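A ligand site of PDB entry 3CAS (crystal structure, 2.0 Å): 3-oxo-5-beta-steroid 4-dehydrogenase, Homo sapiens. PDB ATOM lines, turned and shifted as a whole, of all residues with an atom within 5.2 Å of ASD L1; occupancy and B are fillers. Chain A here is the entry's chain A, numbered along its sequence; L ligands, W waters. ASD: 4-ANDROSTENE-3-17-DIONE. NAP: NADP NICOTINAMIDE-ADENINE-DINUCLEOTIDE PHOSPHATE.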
ATOM      1  N   TYR A  26      18.957 -25.706  19.993  1.00  0.00           N
ATOM      2  CA  TYR A  26      19.253 -24.313  20.206  1.00  0.00           C
ATOM      3  C   TYR A  26      18.323 -23.781  21.291  1.00  0.00           C
ATOM      4  O   TYR A  26      17.145 -24.151  21.328  1.00  0.00           O
ATOM      5  CB  TYR A  26      19.033 -23.449  18.973  1.00  0.00           C
ATOM      6  CG  TYR A  26      19.227 -21.977  19.298  1.00  0.00           C
ATOM      7  CD1 TYR A  26      20.498 -21.421  19.370  1.00  0.00           C
ATOM      8  CD2 TYR A  26      18.143 -21.187  19.686  1.00  0.00           C
ATOM      9  CE1 TYR A  26      20.702 -20.122  19.819  1.00  0.00           C
ATOM     10  CE2 TYR A  26      18.331 -19.881  20.137  1.00  0.00           C
ATOM     11  CZ  TYR A  26      19.612 -19.361  20.203  1.00  0.00           C
ATOM     12  OH  TYR A  26      19.814 -18.088  20.672  1.00  0.00           O
ATOM     13  N   ILE A  57      28.399 -23.056  18.577  1.00  0.00           N
ATOM     14  CA  ILE A  57      27.924 -21.705  18.857  1.00  0.00           C
ATOM     15  C   ILE A  57      26.623 -21.612  19.659  1.00  0.00           C
ATOM     16  O   ILE A  57      26.221 -20.521  20.053  1.00  0.00           O
ATOM     17  CB  ILE A  57      27.796 -20.842  17.573  1.00  0.00           C
ATOM     18  CG1 ILE A  57      26.665 -21.346  16.682  1.00  0.00           C
ATOM     19  CG2 ILE A  57      29.103 -20.859  16.815  1.00  0.00           C
ATOM     20  CD1 ILE A  57      26.392 -20.424  15.487  1.00  0.00           C
ATOM     21  N   TYR A  58      25.978 -22.748  19.903  1.00  0.00           N
ATOM     22  CA  TYR A  58      24.748 -22.738  20.696  1.00  0.00           C
ATOM     23  C   TYR A  58      25.153 -22.628  22.179  1.00  0.00           C
ATOM     24  O   TYR A  58      24.322 -22.356  23.045  1.00  0.00           O
ATOM     25  CB  TYR A  58      23.931 -24.026  20.465  1.00  0.00           C
ATOM     26  CG  TYR A  58      23.346 -24.158  19.063  1.00  0.00           C
ATOM     27  CD1 TYR A  58      22.725 -25.356  18.664  1.00  0.00           C
ATOM     28  CD2 TYR A  58      23.439 -23.117  18.128  1.00  0.00           C
ATOM     29  CE1 TYR A  58      22.210 -25.509  17.369  1.00  0.00           C
ATOM     30  CE2 TYR A  58      22.933 -23.266  16.834  1.00  0.00           C
ATOM     31  CZ  TYR A  58      22.329 -24.459  16.452  1.00  0.00           C
ATOM     32  OH  TYR A  58      21.891 -24.626  15.159  1.00  0.00           O
ATOM     33  N   TRP A  89      31.024 -22.889  12.056  1.00  0.00           N
ATOM     34  CA  TRP A  89      30.557 -21.508  11.962  1.00  0.00           C
ATOM     35  C   TRP A  89      31.365 -20.598  11.022  1.00  0.00           C
ATOM     36  O   TRP A  89      32.531 -20.856  10.716  1.00  0.00           O
ATOM     37  CB  TRP A  89      30.466 -20.875  13.366  1.00  0.00           C
ATOM     38  CG  TRP A  89      29.909 -19.461  13.382  1.00  0.00           C
ATOM     39  CD1 TRP A  89      30.534 -18.347  13.871  1.00  0.00           C
ATOM     40  CD2 TRP A  89      28.663 -19.012  12.829  1.00  0.00           C
ATOM     41  NE1 TRP A  89      29.750 -17.230  13.659  1.00  0.00           N
ATOM     42  CE2 TRP A  89      28.599 -17.614  13.026  1.00  0.00           C
ATOM     43  CE3 TRP A  89      27.591 -19.665  12.201  1.00  0.00           C
ATOM     44  CZ2 TRP A  89      27.507 -16.844  12.604  1.00  0.00           C
ATOM     45  CZ3 TRP A  89      26.498 -18.895  11.779  1.00  0.00           C
ATOM     46  CH2 TRP A  89      26.471 -17.501  11.982  1.00  0.00           C
ATOM     47  N   GLU A 120      27.908 -24.301   8.504  1.00  0.00           N
ATOM     48  CA  GLU A 120      26.719 -23.638   9.054  1.00  0.00           C
ATOM     49  C   GLU A 120      26.051 -22.604   8.154  1.00  0.00           C
ATOM     50  O   GLU A 120      24.820 -22.560   8.076  1.00  0.00           O
ATOM     51  CB  GLU A 120      27.081 -23.027  10.416  1.00  0.00           C
ATOM     52  CG  GLU A 120      25.924 -22.964  11.381  1.00  0.00           C
ATOM     53  CD  GLU A 120      26.362 -23.010  12.843  1.00  0.00           C
ATOM     54  OE1 GLU A 120      27.591 -23.017  13.101  1.00  0.00           O
ATOM     55  OE2 GLU A 120      25.484 -23.040  13.731  1.00  0.00           O
ATOM     56  N   TYR A 132      29.841 -13.210  16.688  1.00  0.00           N
ATOM     57  CA  TYR A 132      29.235 -12.186  15.852  1.00  0.00           C
ATOM     58  C   TYR A 132      30.124 -10.932  15.897  1.00  0.00           C
ATOM     59  O   TYR A 132      29.844  -9.984  16.625  1.00  0.00           O
ATOM     60  CB  TYR A 132      27.832 -11.852  16.351  1.00  0.00           C
ATOM     61  CG  TYR A 132      26.934 -13.058  16.491  1.00  0.00           C
ATOM     62  CD1 TYR A 132      26.565 -13.542  17.748  1.00  0.00           C
ATOM     63  CD2 TYR A 132      26.473 -13.731  15.362  1.00  0.00           C
ATOM     64  CE1 TYR A 132      25.750 -14.666  17.882  1.00  0.00           C
ATOM     65  CE2 TYR A 132      25.662 -14.858  15.486  1.00  0.00           C
ATOM     66  CZ  TYR A 132      25.303 -15.316  16.739  1.00  0.00           C
ATOM     67  OH  TYR A 132      24.510 -16.428  16.854  1.00  0.00           O
ATOM     68  N   TYR A 219      15.185 -27.209   9.382  1.00  0.00           N
ATOM     69  CA  TYR A 219      15.394 -26.617  10.698  1.00  0.00           C
ATOM     70  C   TYR A 219      14.153 -25.761  10.995  1.00  0.00           C
ATOM     71  O   TYR A 219      13.362 -25.485  10.079  1.00  0.00           O
ATOM     72  CB  TYR A 219      16.742 -25.854  10.796  1.00  0.00           C
ATOM     73  CG  TYR A 219      16.944 -24.551  10.028  1.00  0.00           C
ATOM     74  CD1 TYR A 219      16.187 -23.407  10.311  1.00  0.00           C
ATOM     75  CD2 TYR A 219      18.027 -24.413   9.153  1.00  0.00           C
ATOM     76  CE1 TYR A 219      16.512 -22.156   9.752  1.00  0.00           C
ATOM     77  CE2 TYR A 219      18.368 -23.169   8.592  1.00  0.00           C
ATOM     78  CZ  TYR A 219      17.611 -22.035   8.901  1.00  0.00           C
ATOM     79  OH  TYR A 219      17.984 -20.802   8.381  1.00  0.00           O
ATOM     80  N   SER A 220      13.960 -25.366  12.247  1.00  0.00           N
ATOM     81  CA  SER A 220      12.772 -24.597  12.633  1.00  0.00           C
ATOM     82  C   SER A 220      11.530 -25.222  11.968  1.00  0.00           C
ATOM     83  O   SER A 220      10.688 -24.514  11.412  1.00  0.00           O
ATOM     84  CB  SER A 220      12.897 -23.138  12.188  1.00  0.00           C
ATOM     85  OG  SER A 220      13.969 -22.501  12.856  1.00  0.00           O
ATOM     86  N   THR A 224       9.938 -21.885  14.420  1.00  0.00           N
ATOM     87  CA  THR A 224      10.785 -21.143  15.367  1.00  0.00           C
ATOM     88  C   THR A 224      10.141 -20.782  16.692  1.00  0.00           C
ATOM     89  O   THR A 224       8.923 -20.902  16.862  1.00  0.00           O
ATOM     90  CB  THR A 224      11.329 -19.796  14.786  1.00  0.00           C
ATOM     91  OG1 THR A 224      10.313 -18.788  14.893  1.00  0.00           O
ATOM     92  CG2 THR A 224      11.754 -19.943  13.335  1.00  0.00           C
ATOM     93  N   SER A 225      10.969 -20.342  17.638  1.00  0.00           N
ATOM     94  CA  SER A 225      10.484 -19.929  18.955  1.00  0.00           C
ATOM     95  C   SER A 225       9.971 -18.502  18.847  1.00  0.00           C
ATOM     96  O   SER A 225       9.492 -17.926  19.832  1.00  0.00           O
ATOM     97  CB  SER A 225      11.630 -19.977  19.960  1.00  0.00           C
ATOM     98  OG  SER A 225      12.585 -18.967  19.687  1.00  0.00           O
ATOM     99  N   ARG A 226      10.069 -17.932  17.650  1.00  0.00           N
ATOM    100  CA  ARG A 226       9.596 -16.577  17.381  1.00  0.00           C
ATOM    101  C   ARG A 226      10.275 -15.490  18.222  1.00  0.00           C
ATOM    102  O   ARG A 226       9.591 -14.649  18.829  1.00  0.00           O
ATOM    103  CB  ARG A 226       8.073 -16.497  17.532  1.00  0.00           C
ATOM    104  CG  ARG A 226       7.303 -17.416  16.579  1.00  0.00           C
ATOM    105  CD  ARG A 226       5.785 -17.344  16.781  1.00  0.00           C
ATOM    106  NE  ARG A 226       5.223 -16.054  16.395  1.00  0.00           N
ATOM    107  CZ  ARG A 226       5.012 -15.661  15.143  1.00  0.00           C
ATOM    108  NH1 ARG A 226       5.315 -16.452  14.127  1.00  0.00           N
ATOM    109  NH2 ARG A 226       4.500 -14.455  14.899  1.00  0.00           N
ATOM    110  N   ASN A 227      11.597 -15.499  18.269  1.00  0.00           N
ATOM    111  CA  ASN A 227      12.338 -14.481  19.002  1.00  0.00           C
ATOM    112  C   ASN A 227      12.511 -13.304  18.051  1.00  0.00           C
ATOM    113  O   ASN A 227      13.166 -13.420  17.008  1.00  0.00           O
ATOM    114  CB  ASN A 227      13.710 -15.020  19.424  1.00  0.00           C
ATOM    115  CG  ASN A 227      14.490 -14.011  20.268  1.00  0.00           C
ATOM    116  OD1 ASN A 227      14.584 -12.833  19.936  1.00  0.00           O
ATOM    117  ND2 ASN A 227      15.060 -14.488  21.370  1.00  0.00           N
ATOM    118  N   TRP A 230      15.549 -12.580  15.602  1.00  0.00           N
ATOM    119  CA  TRP A 230      15.802 -13.320  14.364  1.00  0.00           C
ATOM    120  C   TRP A 230      14.555 -13.586  13.555  1.00  0.00           C
ATOM    121  O   TRP A 230      14.638 -13.821  12.348  1.00  0.00           O
ATOM    122  CB  TRP A 230      16.457 -14.656  14.658  1.00  0.00           C
ATOM    123  CG  TRP A 230      17.667 -14.558  15.478  1.00  0.00           C
ATOM    124  CD1 TRP A 230      17.738 -14.558  16.847  1.00  0.00           C
ATOM    125  CD2 TRP A 230      19.012 -14.424  15.012  1.00  0.00           C
ATOM    126  NE1 TRP A 230      19.045 -14.427  17.250  1.00  0.00           N
ATOM    127  CE2 TRP A 230      19.849 -14.344  16.139  1.00  0.00           C
ATOM    128  CE3 TRP A 230      19.591 -14.350  13.730  1.00  0.00           C
ATOM    129  CZ2 TRP A 230      21.234 -14.198  16.042  1.00  0.00           C
ATOM    130  CZ3 TRP A 230      20.967 -14.208  13.631  1.00  0.00           C
ATOM    131  CH2 TRP A 230      21.780 -14.137  14.785  1.00  0.00           C
ATOM    132  N   VAL A 231      13.400 -13.588  14.201  1.00  0.00           N
ATOM    133  CA  VAL A 231      12.187 -13.910  13.485  1.00  0.00           C
ATOM    134  C   VAL A 231      11.321 -12.786  12.996  1.00  0.00           C
ATOM    135  O   VAL A 231      11.025 -11.826  13.712  1.00  0.00           O
ATOM    136  CB  VAL A 231      11.299 -14.877  14.298  1.00  0.00           C
ATOM    137  CG1 VAL A 231       9.968 -15.091  13.584  1.00  0.00           C
ATOM    138  CG2 VAL A 231      12.014 -16.197  14.440  1.00  0.00           C
ATOM    139  N   VAL A 309      13.000 -16.881   9.048  1.00  0.00           N
ATOM    140  CA  VAL A 309      14.407 -16.570   9.277  1.00  0.00           C
ATOM    141  C   VAL A 309      15.059 -15.970   8.029  1.00  0.00           C
ATOM    142  O   VAL A 309      15.500 -16.698   7.129  1.00  0.00           O
ATOM    143  CB  VAL A 309      15.184 -17.837   9.690  1.00  0.00           C
ATOM    144  CG1 VAL A 309      16.608 -17.463  10.110  1.00  0.00           C
ATOM    145  CG2 VAL A 309      14.444 -18.544  10.814  1.00  0.00           C
ATOM    146  N   LEU A 311      17.627 -13.442   8.240  1.00  0.00           N
ATOM    147  CA  LEU A 311      19.010 -13.037   8.505  1.00  0.00           C
ATOM    148  C   LEU A 311      19.357 -11.719   7.783  1.00  0.00           C
ATOM    149  O   LEU A 311      20.465 -11.558   7.265  1.00  0.00           O
ATOM    150  CB  LEU A 311      19.976 -14.128   8.040  1.00  0.00           C
ATOM    151  CG  LEU A 311      19.722 -15.566   8.537  1.00  0.00           C
ATOM    152  CD1 LEU A 311      20.720 -16.505   7.858  1.00  0.00           C
ATOM    153  CD2 LEU A 311      19.830 -15.650  10.056  1.00  0.00           C
ATOM    154  N   TRP A 314      22.740  -9.610   7.518  1.00  0.00           N
ATOM    155  CA  TRP A 314      23.880  -9.987   6.683  1.00  0.00           C
ATOM    156  C   TRP A 314      23.546  -9.967   5.182  1.00  0.00           C
ATOM    157  O   TRP A 314      24.228 -10.606   4.387  1.00  0.00           O
ATOM    158  CB  TRP A 314      24.383 -11.401   7.067  1.00  0.00           C
ATOM    159  CG  TRP A 314      24.739 -11.553   8.533  1.00  0.00           C
ATOM    160  CD1 TRP A 314      25.445 -10.677   9.302  1.00  0.00           C
ATOM    161  CD2 TRP A 314      24.449 -12.684   9.372  1.00  0.00           C
ATOM    162  NE1 TRP A 314      25.612 -11.182  10.564  1.00  0.00           N
ATOM    163  CE2 TRP A 314      25.013 -12.417  10.635  1.00  0.00           C
ATOM    164  CE3 TRP A 314      23.765 -13.893   9.179  1.00  0.00           C
ATOM    165  CZ2 TRP A 314      24.921 -13.308  11.711  1.00  0.00           C
ATOM    166  CZ3 TRP A 314      23.678 -14.786  10.246  1.00  0.00           C
ATOM    167  CH2 TRP A 314      24.251 -14.489  11.491  1.00  0.00           C
HETATM  168  C1  ASD L   1      16.995 -18.108  17.597  1.00  0.00           C
HETATM  169  C10 ASD L   1      17.336 -18.912  16.282  1.00  0.00           C
HETATM  170  C11 ASD L   1      19.888 -18.681  16.705  1.00  0.00           C
HETATM  171  C12 ASD L   1      21.248 -18.140  16.144  1.00  0.00           C
HETATM  172  C13 ASD L   1      21.589 -18.649  14.721  1.00  0.00           C
HETATM  173  C14 ASD L   1      20.377 -18.258  13.837  1.00  0.00           C
HETATM  174  C15 ASD L   1      20.831 -18.674  12.406  1.00  0.00           C
HETATM  175  C16 ASD L   1      22.174 -17.901  12.394  1.00  0.00           C
HETATM  176  C17 ASD L   1      22.629 -17.890  13.900  1.00  0.00           C
HETATM  177  C18 ASD L   1      21.949 -20.151  14.814  1.00  0.00           C
HETATM  178  C19 ASD L   1      17.270 -20.422  16.587  1.00  0.00           C
HETATM  179  C2  ASD L   1      15.513 -18.113  18.095  1.00  0.00           C
HETATM  180  C3  ASD L   1      14.498 -17.883  16.940  1.00  0.00           C
HETATM  181  C4  ASD L   1      14.822 -18.140  15.591  1.00  0.00           C
HETATM  182  C5  ASD L   1      16.226 -18.656  15.227  1.00  0.00           C
HETATM  183  C6  ASD L   1      16.502 -18.967  13.751  1.00  0.00           C
HETATM  184  C7  ASD L   1      17.889 -18.380  13.276  1.00  0.00           C
HETATM  185  C8  ASD L   1      19.006 -18.858  14.277  1.00  0.00           C
HETATM  186  C9  ASD L   1      18.694 -18.357  15.750  1.00  0.00           C
HETATM  187  O1  ASD L   1      13.371 -17.475  17.220  1.00  0.00           O
HETATM  188  O2  ASD L   1      23.651 -17.370  14.349  1.00  0.00           O
HETATM  189  PA  NAP L   2      11.371 -25.071  16.221  1.00  0.00           P
HETATM  190  O1A NAP L   2      10.483 -24.666  15.103  1.00  0.00           O
HETATM  191  O2A NAP L   2      11.911 -26.448  16.241  1.00  0.00           O
HETATM  192  O5B NAP L   2      10.613 -24.781  17.662  1.00  0.00           O
HETATM  193  C5B NAP L   2      10.453 -23.461  18.281  1.00  0.00           C
HETATM  194  C4B NAP L   2       9.687 -23.581  19.627  1.00  0.00           C
HETATM  195  O4B NAP L   2       8.618 -24.558  19.542  1.00  0.00           O
HETATM  196  C3B NAP L   2      10.512 -24.070  20.819  1.00  0.00           C
HETATM  197  O3B NAP L   2      11.034 -22.965  21.530  1.00  0.00           O
HETATM  198  C2B NAP L   2       9.572 -24.973  21.655  1.00  0.00           C
HETATM  199  O2B NAP L   2       9.315 -24.587  23.009  1.00  0.00           O
HETATM  200  C1B NAP L   2       8.296 -25.020  20.846  1.00  0.00           C
HETATM  201  N9A NAP L   2       7.671 -26.334  20.705  1.00  0.00           N
HETATM  202  C8A NAP L   2       8.305 -27.559  20.549  1.00  0.00           C
HETATM  203  N7A NAP L   2       7.458 -28.566  20.432  1.00  0.00           N
HETATM  204  C5A NAP L   2       6.230 -27.987  20.526  1.00  0.00           C
HETATM  205  C6A NAP L   2       4.900 -28.509  20.474  1.00  0.00           C
HETATM  206  N6A NAP L   2       4.688 -29.824  20.314  1.00  0.00           N
HETATM  207  N1A NAP L   2       3.843 -27.620  20.597  1.00  0.00           N
HETATM  208  C2A NAP L   2       4.057 -26.268  20.756  1.00  0.00           C
HETATM  209  N3A NAP L   2       5.295 -25.664  20.808  1.00  0.00           N
HETATM  210  C4A NAP L   2       6.337 -26.592  20.693  1.00  0.00           C
HETATM  211  O3  NAP L   2      12.583 -24.022  16.214  1.00  0.00           O
HETATM  212  PN  NAP L   2      14.169 -24.040  16.101  1.00  0.00           P
HETATM  213  O1N NAP L   2      14.686 -24.350  17.441  1.00  0.00           O
HETATM  214  O2N NAP L   2      14.561 -22.701  15.539  1.00  0.00           O
HETATM  215  O5D NAP L   2      14.581 -25.165  15.059  1.00  0.00           O
HETATM  216  C5D NAP L   2      14.894 -26.541  15.418  1.00  0.00           C
HETATM  217  C4D NAP L   2      16.376 -26.763  15.438  1.00  0.00           C
HETATM  218  O4D NAP L   2      16.955 -26.465  14.120  1.00  0.00           O
HETATM  219  C3D NAP L   2      17.233 -25.889  16.375  1.00  0.00           C
HETATM  220  O3D NAP L   2      17.066 -26.116  17.762  1.00  0.00           O
HETATM  221  C2D NAP L   2      18.618 -26.111  15.783  1.00  0.00           C
HETATM  222  O2D NAP L   2      19.158 -27.345  16.288  1.00  0.00           O
HETATM  223  C1D NAP L   2      18.313 -26.095  14.273  1.00  0.00           C
HETATM  224  N1N NAP L   2      18.531 -24.756  13.603  1.00  0.00           N
HETATM  225  C2N NAP L   2      19.573 -24.718  12.690  1.00  0.00           C
HETATM  226  C3N NAP L   2      19.883 -23.529  11.987  1.00  0.00           C
HETATM  227  C7N NAP L   2      21.002 -23.474  10.997  1.00  0.00           C
HETATM  228  O7N NAP L   2      21.343 -22.402  10.499  1.00  0.00           O
HETATM  229  N7N NAP L   2      21.585 -24.634  10.647  1.00  0.00           N
HETATM  230  C4N NAP L   2      19.084 -22.342  12.247  1.00  0.00           C
HETATM  231  C5N NAP L   2      18.017 -22.389  13.187  1.00  0.00           C
HETATM  232  C6N NAP L   2      17.731 -23.586  13.857  1.00  0.00           C
HETATM  233  P2B NAP L   2       9.665 -25.589  24.266  1.00  0.00           P
HETATM  234  O1X NAP L   2      11.152 -25.891  24.203  1.00  0.00           O
HETATM  235  O2X NAP L   2       9.207 -24.778  25.461  1.00  0.00           O
HETATM  236  O3X NAP L   2       8.839 -26.830  24.060  1.00  0.00           O
HETATM  237  O   HOH W   1      23.022 -22.992  13.256  1.00  0.00           O
HETATM  238  O   HOH W   2      13.729 -20.993  17.599  1.00  0.00           O
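OH of Tyr 132 lies within hydrogen-bond range of O2 of ASD L1.
The backbone NH (N) of Asn 227 lies within hydrogen-bond range of an oxygen (O1) of ASD L1 (2.9 Å).
OG of Ser 225 lies within hydrogen-bond range of O1 of ASD L1, 3.0 Å away.
The backbone NH (N) of Arg 226 sits at hydrogen-bond distance from an oxygen (O1) of ASD L1 (3.4 Å).
N of Tyr 26 is in hydrogen-bond range of O3D of NAP L2, at 3.0 Å.
The backbone NH (N) of Thr 224 sits at hydrogen-bond distance from an oxygen (O1A) of NAP L2, 2.9 Å away.
N of Ser 220 lies within hydrogen-bond range of O5D of NAP L2 (2.9 Å).
OG of Ser 220 sits at hydrogen-bond distance from O2N of NAP L2.
The backbone NH of Arg 226 is in hydrogen-bond range of the side-chain hydroxyl of Thr 224 (2.9 Å).
Tyr 26 touches ASD L1.
Tyr 58 touches ASD L1.
Trp 89 touches ASD L1.
Thr 224 touches ASD L1.
Trp 230 touches ASD L1.
CG2 of Val 231 touches O1 of ASD L1, 3.3 Å away.
CG1 of Val 309 touches C7 of ASD L1 (3.5 Å).
CD2 of Leu 311 touches C15 of ASD L1 (3.96 Å).
Hydrophobic or aromatic side chains within 4 Å of ASD L1: Tyr 26, Tyr 58, Trp 89, Tyr 132, Trp 230, Val 231, Val 309 and Leu 311.
Water W2 bridges O2N of NAP L2 (2.8 Å) and N of Ser 225 (2.8 Å).
Water W1 lies within hydrogen-bond range of the side-chain carboxylate (OE2) of Glu 120 (2.5 Å), the side-chain hydroxyl (OH) of Tyr 58 (2.8 Å) and an oxygen (O7N) of NAP L2 (3.3 Å).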
